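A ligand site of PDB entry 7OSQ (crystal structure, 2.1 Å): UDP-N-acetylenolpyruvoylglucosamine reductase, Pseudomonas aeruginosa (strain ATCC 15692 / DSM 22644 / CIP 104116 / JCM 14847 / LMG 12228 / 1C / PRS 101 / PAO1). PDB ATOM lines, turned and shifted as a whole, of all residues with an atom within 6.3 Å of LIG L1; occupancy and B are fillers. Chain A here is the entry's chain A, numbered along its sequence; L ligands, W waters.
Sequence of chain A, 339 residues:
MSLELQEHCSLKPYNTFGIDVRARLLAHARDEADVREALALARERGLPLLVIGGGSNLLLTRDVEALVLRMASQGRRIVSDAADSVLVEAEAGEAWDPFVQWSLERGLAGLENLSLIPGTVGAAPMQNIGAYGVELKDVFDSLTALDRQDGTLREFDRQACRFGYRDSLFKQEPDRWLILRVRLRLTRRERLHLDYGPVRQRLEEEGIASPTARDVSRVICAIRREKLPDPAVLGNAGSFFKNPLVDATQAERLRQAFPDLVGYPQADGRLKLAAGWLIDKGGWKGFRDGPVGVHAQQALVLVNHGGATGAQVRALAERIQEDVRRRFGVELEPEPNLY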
ATOM      1  N   GLY A 130      17.958  21.293  23.823  1.00  0.00           N
ATOM      2  CA  GLY A 130      17.832  20.376  24.942  1.00  0.00           C
ATOM      3  C   GLY A 130      19.067  19.507  25.048  1.00  0.00           C
ATOM      4  O   GLY A 130      19.678  19.135  24.041  1.00  0.00           O
ATOM      5  N   ALA A 131      19.390  19.145  26.283  1.00  0.00           N
ATOM      6  CA  ALA A 131      20.515  18.249  26.524  1.00  0.00           C
ATOM      7  C   ALA A 131      20.453  17.792  27.966  1.00  0.00           C
ATOM      8  O   ALA A 131      19.992  18.537  28.843  1.00  0.00           O
ATOM      9  CB  ALA A 131      21.866  18.936  26.259  1.00  0.00           C
ATOM     10  N   TYR A 132      20.888  16.546  28.187  1.00  0.00           N
ATOM     11  CA  TYR A 132      21.022  15.947  29.516  1.00  0.00           C
ATOM     12  C   TYR A 132      19.794  16.223  30.380  1.00  0.00           C
ATOM     13  O   TYR A 132      19.890  16.649  31.514  1.00  0.00           O
ATOM     14  CB  TYR A 132      22.321  16.440  30.193  1.00  0.00           C
ATOM     15  CG  TYR A 132      23.530  16.054  29.361  1.00  0.00           C
ATOM     16  CD1 TYR A 132      24.026  14.752  29.375  1.00  0.00           C
ATOM     17  CD2 TYR A 132      24.149  16.981  28.532  1.00  0.00           C
ATOM     18  CE1 TYR A 132      25.116  14.380  28.588  1.00  0.00           C
ATOM     19  CE2 TYR A 132      25.238  16.619  27.724  1.00  0.00           C
ATOM     20  CZ  TYR A 132      25.718  15.315  27.763  1.00  0.00           C
ATOM     21  OH  TYR A 132      26.795  14.938  26.979  1.00  0.00           O
ATOM     22  N   GLY A 133      18.611  15.993  29.786  1.00  0.00           N
ATOM     23  CA  GLY A 133      17.355  16.038  30.502  1.00  0.00           C
ATOM     24  C   GLY A 133      16.709  17.401  30.657  1.00  0.00           C
ATOM     25  O   GLY A 133      15.628  17.487  31.242  1.00  0.00           O
ATOM     26  N   TYR A 165       9.290  18.386  21.401  1.00  0.00           N
ATOM     27  CA  TYR A 165      10.635  17.852  21.377  1.00  0.00           C
ATOM     28  C   TYR A 165      11.426  18.407  20.183  1.00  0.00           C
ATOM     29  O   TYR A 165      11.087  18.133  19.029  1.00  0.00           O
ATOM     30  CB  TYR A 165      10.590  16.327  21.325  1.00  0.00           C
ATOM     31  CG  TYR A 165      11.964  15.715  21.446  1.00  0.00           C
ATOM     32  CD1 TYR A 165      12.521  14.990  20.397  1.00  0.00           C
ATOM     33  CD2 TYR A 165      12.695  15.867  22.609  1.00  0.00           C
ATOM     34  CE1 TYR A 165      13.801  14.430  20.504  1.00  0.00           C
ATOM     35  CE2 TYR A 165      13.975  15.330  22.718  1.00  0.00           C
ATOM     36  CZ  TYR A 165      14.514  14.613  21.674  1.00  0.00           C
ATOM     37  OH  TYR A 165      15.772  14.078  21.820  1.00  0.00           O
ATOM     38  N   ARG A 166      12.477  19.177  20.472  1.00  0.00           N
ATOM     39  CA  ARG A 166      13.240  19.867  19.426  1.00  0.00           C
ATOM     40  C   ARG A 166      12.329  20.558  18.422  1.00  0.00           C
ATOM     41  O   ARG A 166      12.578  20.542  17.209  1.00  0.00           O
ATOM     42  CB  ARG A 166      14.167  18.911  18.680  1.00  0.00           C
ATOM     43  CG  ARG A 166      15.087  18.207  19.578  1.00  0.00           C
ATOM     44  CD  ARG A 166      15.858  19.253  20.332  1.00  0.00           C
ATOM     45  NE  ARG A 166      17.176  18.708  20.544  1.00  0.00           N
ATOM     46  CZ  ARG A 166      17.467  18.029  21.640  1.00  0.00           C
ATOM     47  NH1 ARG A 166      16.530  17.892  22.560  1.00  0.00           N
ATOM     48  NH2 ARG A 166      18.650  17.506  21.786  1.00  0.00           N
ATOM     49  N   ARG A 224      30.835  16.626  27.160  1.00  0.00           N
ATOM     50  CA  ARG A 224      30.590  17.015  25.759  1.00  0.00           C
ATOM     51  C   ARG A 224      31.896  17.118  24.973  1.00  0.00           C
ATOM     52  O   ARG A 224      31.965  16.660  23.823  1.00  0.00           O
ATOM     53  CB  ARG A 224      29.821  18.327  25.697  1.00  0.00           C
ATOM     54  CG  ARG A 224      28.378  18.230  26.209  1.00  0.00           C
ATOM     55  CD  ARG A 224      27.627  19.572  26.081  1.00  0.00           C
ATOM     56  NE  ARG A 224      27.439  19.924  24.663  1.00  0.00           N
ATOM     57  CZ  ARG A 224      26.306  19.762  23.974  1.00  0.00           C
ATOM     58  NH1 ARG A 224      25.225  19.244  24.566  1.00  0.00           N
ATOM     59  NH2 ARG A 224      26.276  20.097  22.688  1.00  0.00           N
ATOM     60  N   LEU A 228      31.699  14.418  21.910  1.00  0.00           N
ATOM     61  CA  LEU A 228      30.974  14.981  20.775  1.00  0.00           C
ATOM     62  C   LEU A 228      31.922  15.624  19.770  1.00  0.00           C
ATOM     63  O   LEU A 228      32.679  16.523  20.137  1.00  0.00           O
ATOM     64  CB  LEU A 228      29.939  16.006  21.243  1.00  0.00           C
ATOM     65  CG  LEU A 228      29.020  15.560  22.374  1.00  0.00           C
ATOM     66  CD1 LEU A 228      27.990  16.649  22.718  1.00  0.00           C
ATOM     67  CD2 LEU A 228      28.349  14.240  22.048  1.00  0.00           C
ATOM     68  N   PRO A 229      31.875  15.219  18.498  1.00  0.00           N
ATOM     69  CA  PRO A 229      32.804  15.784  17.514  1.00  0.00           C
ATOM     70  C   PRO A 229      32.636  17.291  17.386  1.00  0.00           C
ATOM     71  O   PRO A 229      31.525  17.815  17.365  1.00  0.00           O
ATOM     72  CB  PRO A 229      32.425  15.064  16.208  1.00  0.00           C
ATOM     73  CG  PRO A 229      31.636  13.871  16.626  1.00  0.00           C
ATOM     74  CD  PRO A 229      30.937  14.261  17.888  1.00  0.00           C
ATOM     75  N   ASN A 236      29.832  19.038  11.135  1.00  0.00           N
ATOM     76  CA  ASN A 236      28.602  18.364  11.554  1.00  0.00           C
ATOM     77  C   ASN A 236      27.635  19.419  12.087  1.00  0.00           C
ATOM     78  O   ASN A 236      27.980  20.594  12.207  1.00  0.00           O
ATOM     79  CB  ASN A 236      28.855  17.270  12.611  1.00  0.00           C
ATOM     80  CG  ASN A 236      29.192  17.828  13.995  1.00  0.00           C
ATOM     81  OD1 ASN A 236      28.312  18.087  14.823  1.00  0.00           O
ATOM     82  ND2 ASN A 236      30.482  17.982  14.265  1.00  0.00           N
ATOM     83  N   ALA A 237      26.398  18.988  12.361  1.00  0.00           N
ATOM     84  CA  ALA A 237      25.344  19.782  12.980  1.00  0.00           C
ATOM     85  C   ALA A 237      24.850  19.087  14.242  1.00  0.00           C
ATOM     86  O   ALA A 237      23.653  19.174  14.590  1.00  0.00           O
ATOM     87  CB  ALA A 237      24.189  20.036  12.014  1.00  0.00           C
ATOM     88  N   GLY A 238      25.743  18.376  14.908  1.00  0.00           N
ATOM     89  CA  GLY A 238      25.385  17.660  16.121  1.00  0.00           C
ATOM     90  C   GLY A 238      24.551  16.445  15.772  1.00  0.00           C
ATOM     91  O   GLY A 238      24.808  15.792  14.758  1.00  0.00           O
ATOM     92  N   SER A 239      23.570  16.123  16.614  1.00  0.00           N
ATOM     93  CA  SER A 239      22.706  14.984  16.350  1.00  0.00           C
ATOM     94  C   SER A 239      21.848  15.270  15.136  1.00  0.00           C
ATOM     95  O   SER A 239      21.040  16.188  15.151  1.00  0.00           O
ATOM     96  CB  SER A 239      21.813  14.686  17.563  1.00  0.00           C
ATOM     97  OG  SER A 239      20.941  13.602  17.261  1.00  0.00           O
ATOM     98  N   ASN A 243      15.253  11.526  18.522  1.00  0.00           N
ATOM     99  CA  ASN A 243      14.710  10.288  19.067  1.00  0.00           C
ATOM    100  C   ASN A 243      13.230  10.191  18.728  1.00  0.00           C
ATOM    101  O   ASN A 243      12.457  11.089  19.086  1.00  0.00           O
ATOM    102  CB  ASN A 243      14.922  10.219  20.574  1.00  0.00           C
ATOM    103  CG  ASN A 243      16.373  10.035  20.962  1.00  0.00           C
ATOM    104  OD1 ASN A 243      17.171   9.499  20.186  1.00  0.00           O
ATOM    105  ND2 ASN A 243      16.729  10.450  22.179  1.00  0.00           N
ATOM    106  N   GLN A 298      29.590   8.139  17.827  1.00  0.00           N
ATOM    107  CA  GLN A 298      28.305   8.811  17.986  1.00  0.00           C
ATOM    108  C   GLN A 298      27.507   8.547  16.701  1.00  0.00           C
ATOM    109  O   GLN A 298      27.649   9.269  15.715  1.00  0.00           O
ATOM    110  CB  GLN A 298      28.518  10.299  18.239  1.00  0.00           C
ATOM    111  CG  GLN A 298      29.307  10.567  19.526  1.00  0.00           C
ATOM    112  CD  GLN A 298      28.677   9.886  20.733  1.00  0.00           C
ATOM    113  OE1 GLN A 298      27.481  10.040  20.980  1.00  0.00           O
ATOM    114  NE2 GLN A 298      29.472   9.150  21.498  1.00  0.00           N
ATOM    115  N   LEU A 300      24.527   9.026  15.911  1.00  0.00           N
ATOM    116  CA  LEU A 300      23.574  10.066  15.556  1.00  0.00           C
ATOM    117  C   LEU A 300      24.194  11.177  14.703  1.00  0.00           C
ATOM    118  O   LEU A 300      23.448  11.973  14.124  1.00  0.00           O
ATOM    119  CB  LEU A 300      22.982  10.703  16.818  1.00  0.00           C
ATOM    120  CG  LEU A 300      21.987   9.953  17.719  1.00  0.00           C
ATOM    121  CD1 LEU A 300      22.093  10.474  19.124  1.00  0.00           C
ATOM    122  CD2 LEU A 300      20.578  10.108  17.215  1.00  0.00           C
ATOM    123  N   VAL A 301      25.524  11.251  14.615  1.00  0.00           N
ATOM    124  CA  VAL A 301      26.207  12.429  14.100  1.00  0.00           C
ATOM    125  C   VAL A 301      26.669  12.122  12.681  1.00  0.00           C
ATOM    126  O   VAL A 301      27.626  11.365  12.485  1.00  0.00           O
ATOM    127  CB  VAL A 301      27.394  12.846  14.982  1.00  0.00           C
ATOM    128  CG1 VAL A 301      28.034  14.106  14.420  1.00  0.00           C
ATOM    129  CG2 VAL A 301      26.950  13.061  16.455  1.00  0.00           C
ATOM    130  N   GLU A 335      16.920  16.682  12.986  1.00  0.00           N
ATOM    131  CA  GLU A 335      16.976  17.873  13.842  1.00  0.00           C
ATOM    132  C   GLU A 335      17.350  19.121  13.022  1.00  0.00           C
ATOM    133  O   GLU A 335      16.693  20.157  13.166  1.00  0.00           O
ATOM    134  CB  GLU A 335      17.953  17.662  15.026  1.00  0.00           C
ATOM    135  CG  GLU A 335      17.737  18.659  16.167  1.00  0.00           C
ATOM    136  CD  GLU A 335      18.704  18.462  17.333  1.00  0.00           C
ATOM    137  OE1 GLU A 335      19.939  18.558  17.128  1.00  0.00           O
ATOM    138  OE2 GLU A 335      18.230  18.244  18.475  1.00  0.00           O
HETATM  139  C1  LIG L   1      24.041  14.709  23.821  1.00  0.00           C
HETATM  140  C2  LIG L   1      26.138  15.293  19.000  1.00  0.00           C
HETATM  141  C3  LIG L   1      25.788  16.548  19.473  1.00  0.00           C
HETATM  142  C4  LIG L   1      24.737  16.714  20.376  1.00  0.00           C
HETATM  143  C5  LIG L   1      24.054  15.594  20.800  1.00  0.00           C
HETATM  144  C6  LIG L   1      24.394  14.331  20.308  1.00  0.00           C
HETATM  145  C7  LIG L   1      25.432  14.160  19.409  1.00  0.00           C
HETATM  146  C8  LIG L   1      22.892  15.257  22.980  1.00  0.00           C
HETATM  147  C9  LIG L   1      21.529  15.480  23.401  1.00  0.00           C
HETATM  148  C10 LIG L   1      20.872  15.208  24.747  1.00  0.00           C
HETATM  149  N1  LIG L   1      22.925  15.664  21.710  1.00  0.00           N
HETATM  150  N2  LIG L   1      20.882  15.970  22.335  1.00  0.00           N
HETATM  151  N3  LIG L   1      21.721  16.078  21.326  1.00  0.00           N
HETATM  152  O1  LIG L   1      21.541  15.062  25.832  1.00  0.00           O
HETATM  153  O2  LIG L   1      19.609  15.128  24.722  1.00  0.00           O
HETATM  154  P1  LG2 L   2      21.197  28.395  12.840  1.00  0.00           P
HETATM  155  O1  LG2 L   2      21.642  27.059  12.431  1.00  0.00           O
HETATM  156  O2  LG2 L   2      21.891  29.650  12.388  1.00  0.00           O
HETATM  157  O3  LG2 L   2      19.750  28.417  12.382  1.00  0.00           O
HETATM  158  C1  LG2 L   2      18.920  27.248  12.471  1.00  0.00           C
HETATM  159  C2  LG2 L   2      17.544  27.570  12.037  1.00  0.00           C
HETATM  160  O4  LG2 L   2      16.935  28.516  12.943  1.00  0.00           O
HETATM  161  C3  LG2 L   2      17.421  28.181  10.653  1.00  0.00           C
HETATM  162  O5  LG2 L   2      16.161  27.848  10.118  1.00  0.00           O
HETATM  163  C4  LG2 L   2      17.477  29.668  10.960  1.00  0.00           C
HETATM  164  O6  LG2 L   2      16.734  30.409  10.015  1.00  0.00           O
HETATM  165  C5  LG2 L   2      16.743  29.748  12.291  1.00  0.00           C
HETATM  166  N1  LG2 L   2      17.099  30.921  13.104  1.00  0.00           N
HETATM  167  C6  LG2 L   2      18.297  31.296  13.669  1.00  0.00           C
HETATM  168  N2  LG2 L   2      18.258  32.466  14.280  1.00  0.00           N
HETATM  169  C7  LG2 L   2      16.972  32.900  14.085  1.00  0.00           C
HETATM  170  C8  LG2 L   2      16.260  34.070  14.479  1.00  0.00           C
HETATM  171  N3  LG2 L   2      16.804  35.063  15.211  1.00  0.00           N
HETATM  172  N4  LG2 L   2      14.970  34.193  14.117  1.00  0.00           N
HETATM  173  C9  LG2 L   2      14.410  33.218  13.380  1.00  0.00           C
HETATM  174  N5  LG2 L   2      14.972  32.101  12.937  1.00  0.00           N
HETATM  175  C10 LG2 L   2      16.241  31.989  13.326  1.00  0.00           C
HETATM  176  N6  LG2 L   2      20.967  21.118  19.734  1.00  0.00           N
HETATM  177  C11 LG2 L   2      20.362  20.696  20.882  1.00  0.00           C
HETATM  178  O7  LG2 L   2      19.163  20.880  21.069  1.00  0.00           O
HETATM  179  N7  LG2 L   2      21.108  20.055  21.863  1.00  0.00           N
HETATM  180  C12 LG2 L   2      22.454  19.780  21.777  1.00  0.00           C
HETATM  181  O8  LG2 L   2      23.014  19.197  22.698  1.00  0.00           O
HETATM  182  C13 LG2 L   2      23.103  20.221  20.555  1.00  0.00           C
HETATM  183  N8  LG2 L   2      24.381  19.992  20.396  1.00  0.00           N
HETATM  184  C14 LG2 L   2      24.984  20.425  19.228  1.00  0.00           C
HETATM  185  C15 LG2 L   2      26.349  20.177  19.045  1.00  0.00           C
HETATM  186  C16 LG2 L   2      27.002  20.578  17.902  1.00  0.00           C
HETATM  187  C17 LG2 L   2      28.469  20.299  17.762  1.00  0.00           C
HETATM  188  C18 LG2 L   2      26.293  21.231  16.871  1.00  0.00           C
HETATM  189  C19 LG2 L   2      27.020  21.656  15.626  1.00  0.00           C
HETATM  190  C20 LG2 L   2      24.919  21.470  17.036  1.00  0.00           C
HETATM  191  C21 LG2 L   2      24.248  21.077  18.183  1.00  0.00           C
HETATM  192  N9  LG2 L   2      22.873  21.300  18.410  1.00  0.00           N
HETATM  193  C22 LG2 L   2      22.251  20.886  19.563  1.00  0.00           C
HETATM  194  C23 LG2 L   2      22.033  22.000  17.365  1.00  0.00           C
HETATM  195  C24 LG2 L   2      21.391  23.282  17.889  1.00  0.00           C
HETATM  196  O9  LG2 L   2      20.091  23.583  17.361  1.00  0.00           O
HETATM  197  C25 LG2 L   2      22.281  24.444  17.513  1.00  0.00           C
HETATM  198  O10 LG2 L   2      23.550  24.183  18.104  1.00  0.00           O
HETATM  199  C26 LG2 L   2      21.676  25.812  17.834  1.00  0.00           C
HETATM  200  O11 LG2 L   2      20.472  25.794  18.595  1.00  0.00           O
HETATM  201  C27 LG2 L   2      21.282  26.488  16.549  1.00  0.00           C
HETATM  202  O12 LG2 L   2      21.554  27.885  16.688  1.00  0.00           O
HETATM  203  P2  LG2 L   2      22.185  28.690  15.517  1.00  0.00           P
HETATM  204  O13 LG2 L   2      22.065  30.111  16.068  1.00  0.00           O
HETATM  205  O14 LG2 L   2      23.412  28.002  15.115  1.00  0.00           O
HETATM  206  O15 LG2 L   2      21.044  28.476  14.424  1.00  0.00           O
HETATM  207  O   HOH W   1      18.029  15.364  26.887  1.00  0.00           O
HETATM  208  O   HOH W   2      22.240  17.942  18.662  1.00  0.00           O
HETATM  209  O   HOH W   3      28.816  16.607  17.488  1.00  0.00           O
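The backbone NH of Gly 130 lies within hydrogen-bond range of an oxygen (O7) of LG2 L2 (3.0 Å). The backbone carbonyl oxygen (O) of Gly 130 lies within hydrogen-bond range of a nitrogen (N7) of LG2 L2 (2.8 Å). An oxygen (O1) of LIG L1 lies within hydrogen-bond range of the backbone NH (N) of Tyr 132, at 2.9 Å. The guanidinium group of Arg 224 lies within hydrogen-bond range of an oxygen (O8) of LG2 L2 (2.9 Å). NH2 of Arg 166 lies within salt-bridge range of O2 of LIG L1, 3.9 Å away. NE of Arg 166 lies within hydrogen-bond range of O7 of LG2 L2 (3.0 Å).
The guanidinium group (NH2) of Arg 166 sits at hydrogen-bond distance from the backbone carbonyl oxygen (O) of Gly 130, 3.0 Å away. OE2 of Glu 335 lies within salt-bridge range of NH2 of Arg 166 (3.4 Å). The side-chain amide oxygen (OD1) of Asn 236 is in hydrogen-bond range of the backbone NH (N) of Gly 238 (2.6 Å).
Gly 130 touches LIG L1 (O to N2, 3.8 Å). Ala 131 touches LIG L1. Leu 228 touches LIG L1. CA of Gly 238 touches C3 of LIG L1 (3.6 Å). Ser 239 touches LIG L1 (N to C2, 3.6 Å). Val 301 touches LIG L1 (CG2 to C2, 3.5 Å). Hydrophobic or aromatic side chains within 4 Å of LIG L1: Ala 131, Leu 228 and Val 301. Within 4 Å of LIG L1: Gly 130, Ala 131, Tyr 132, Arg 166, Leu 228, Gly 238, Ser 239 and Val 301. The nearest printed residue that does not touch LIG L1 is Arg 224 (4.4 Å).
Water W1 lies within hydrogen-bond range of O2 of LIG L1 (2.7 Å), N of Gly 133 (3.0 Å) and N of Tyr 132 (3.4 Å). Water W3 bridges the backbone carbonyl oxygen of Pro 229 and the side-chain amide oxygen of Asn 236.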
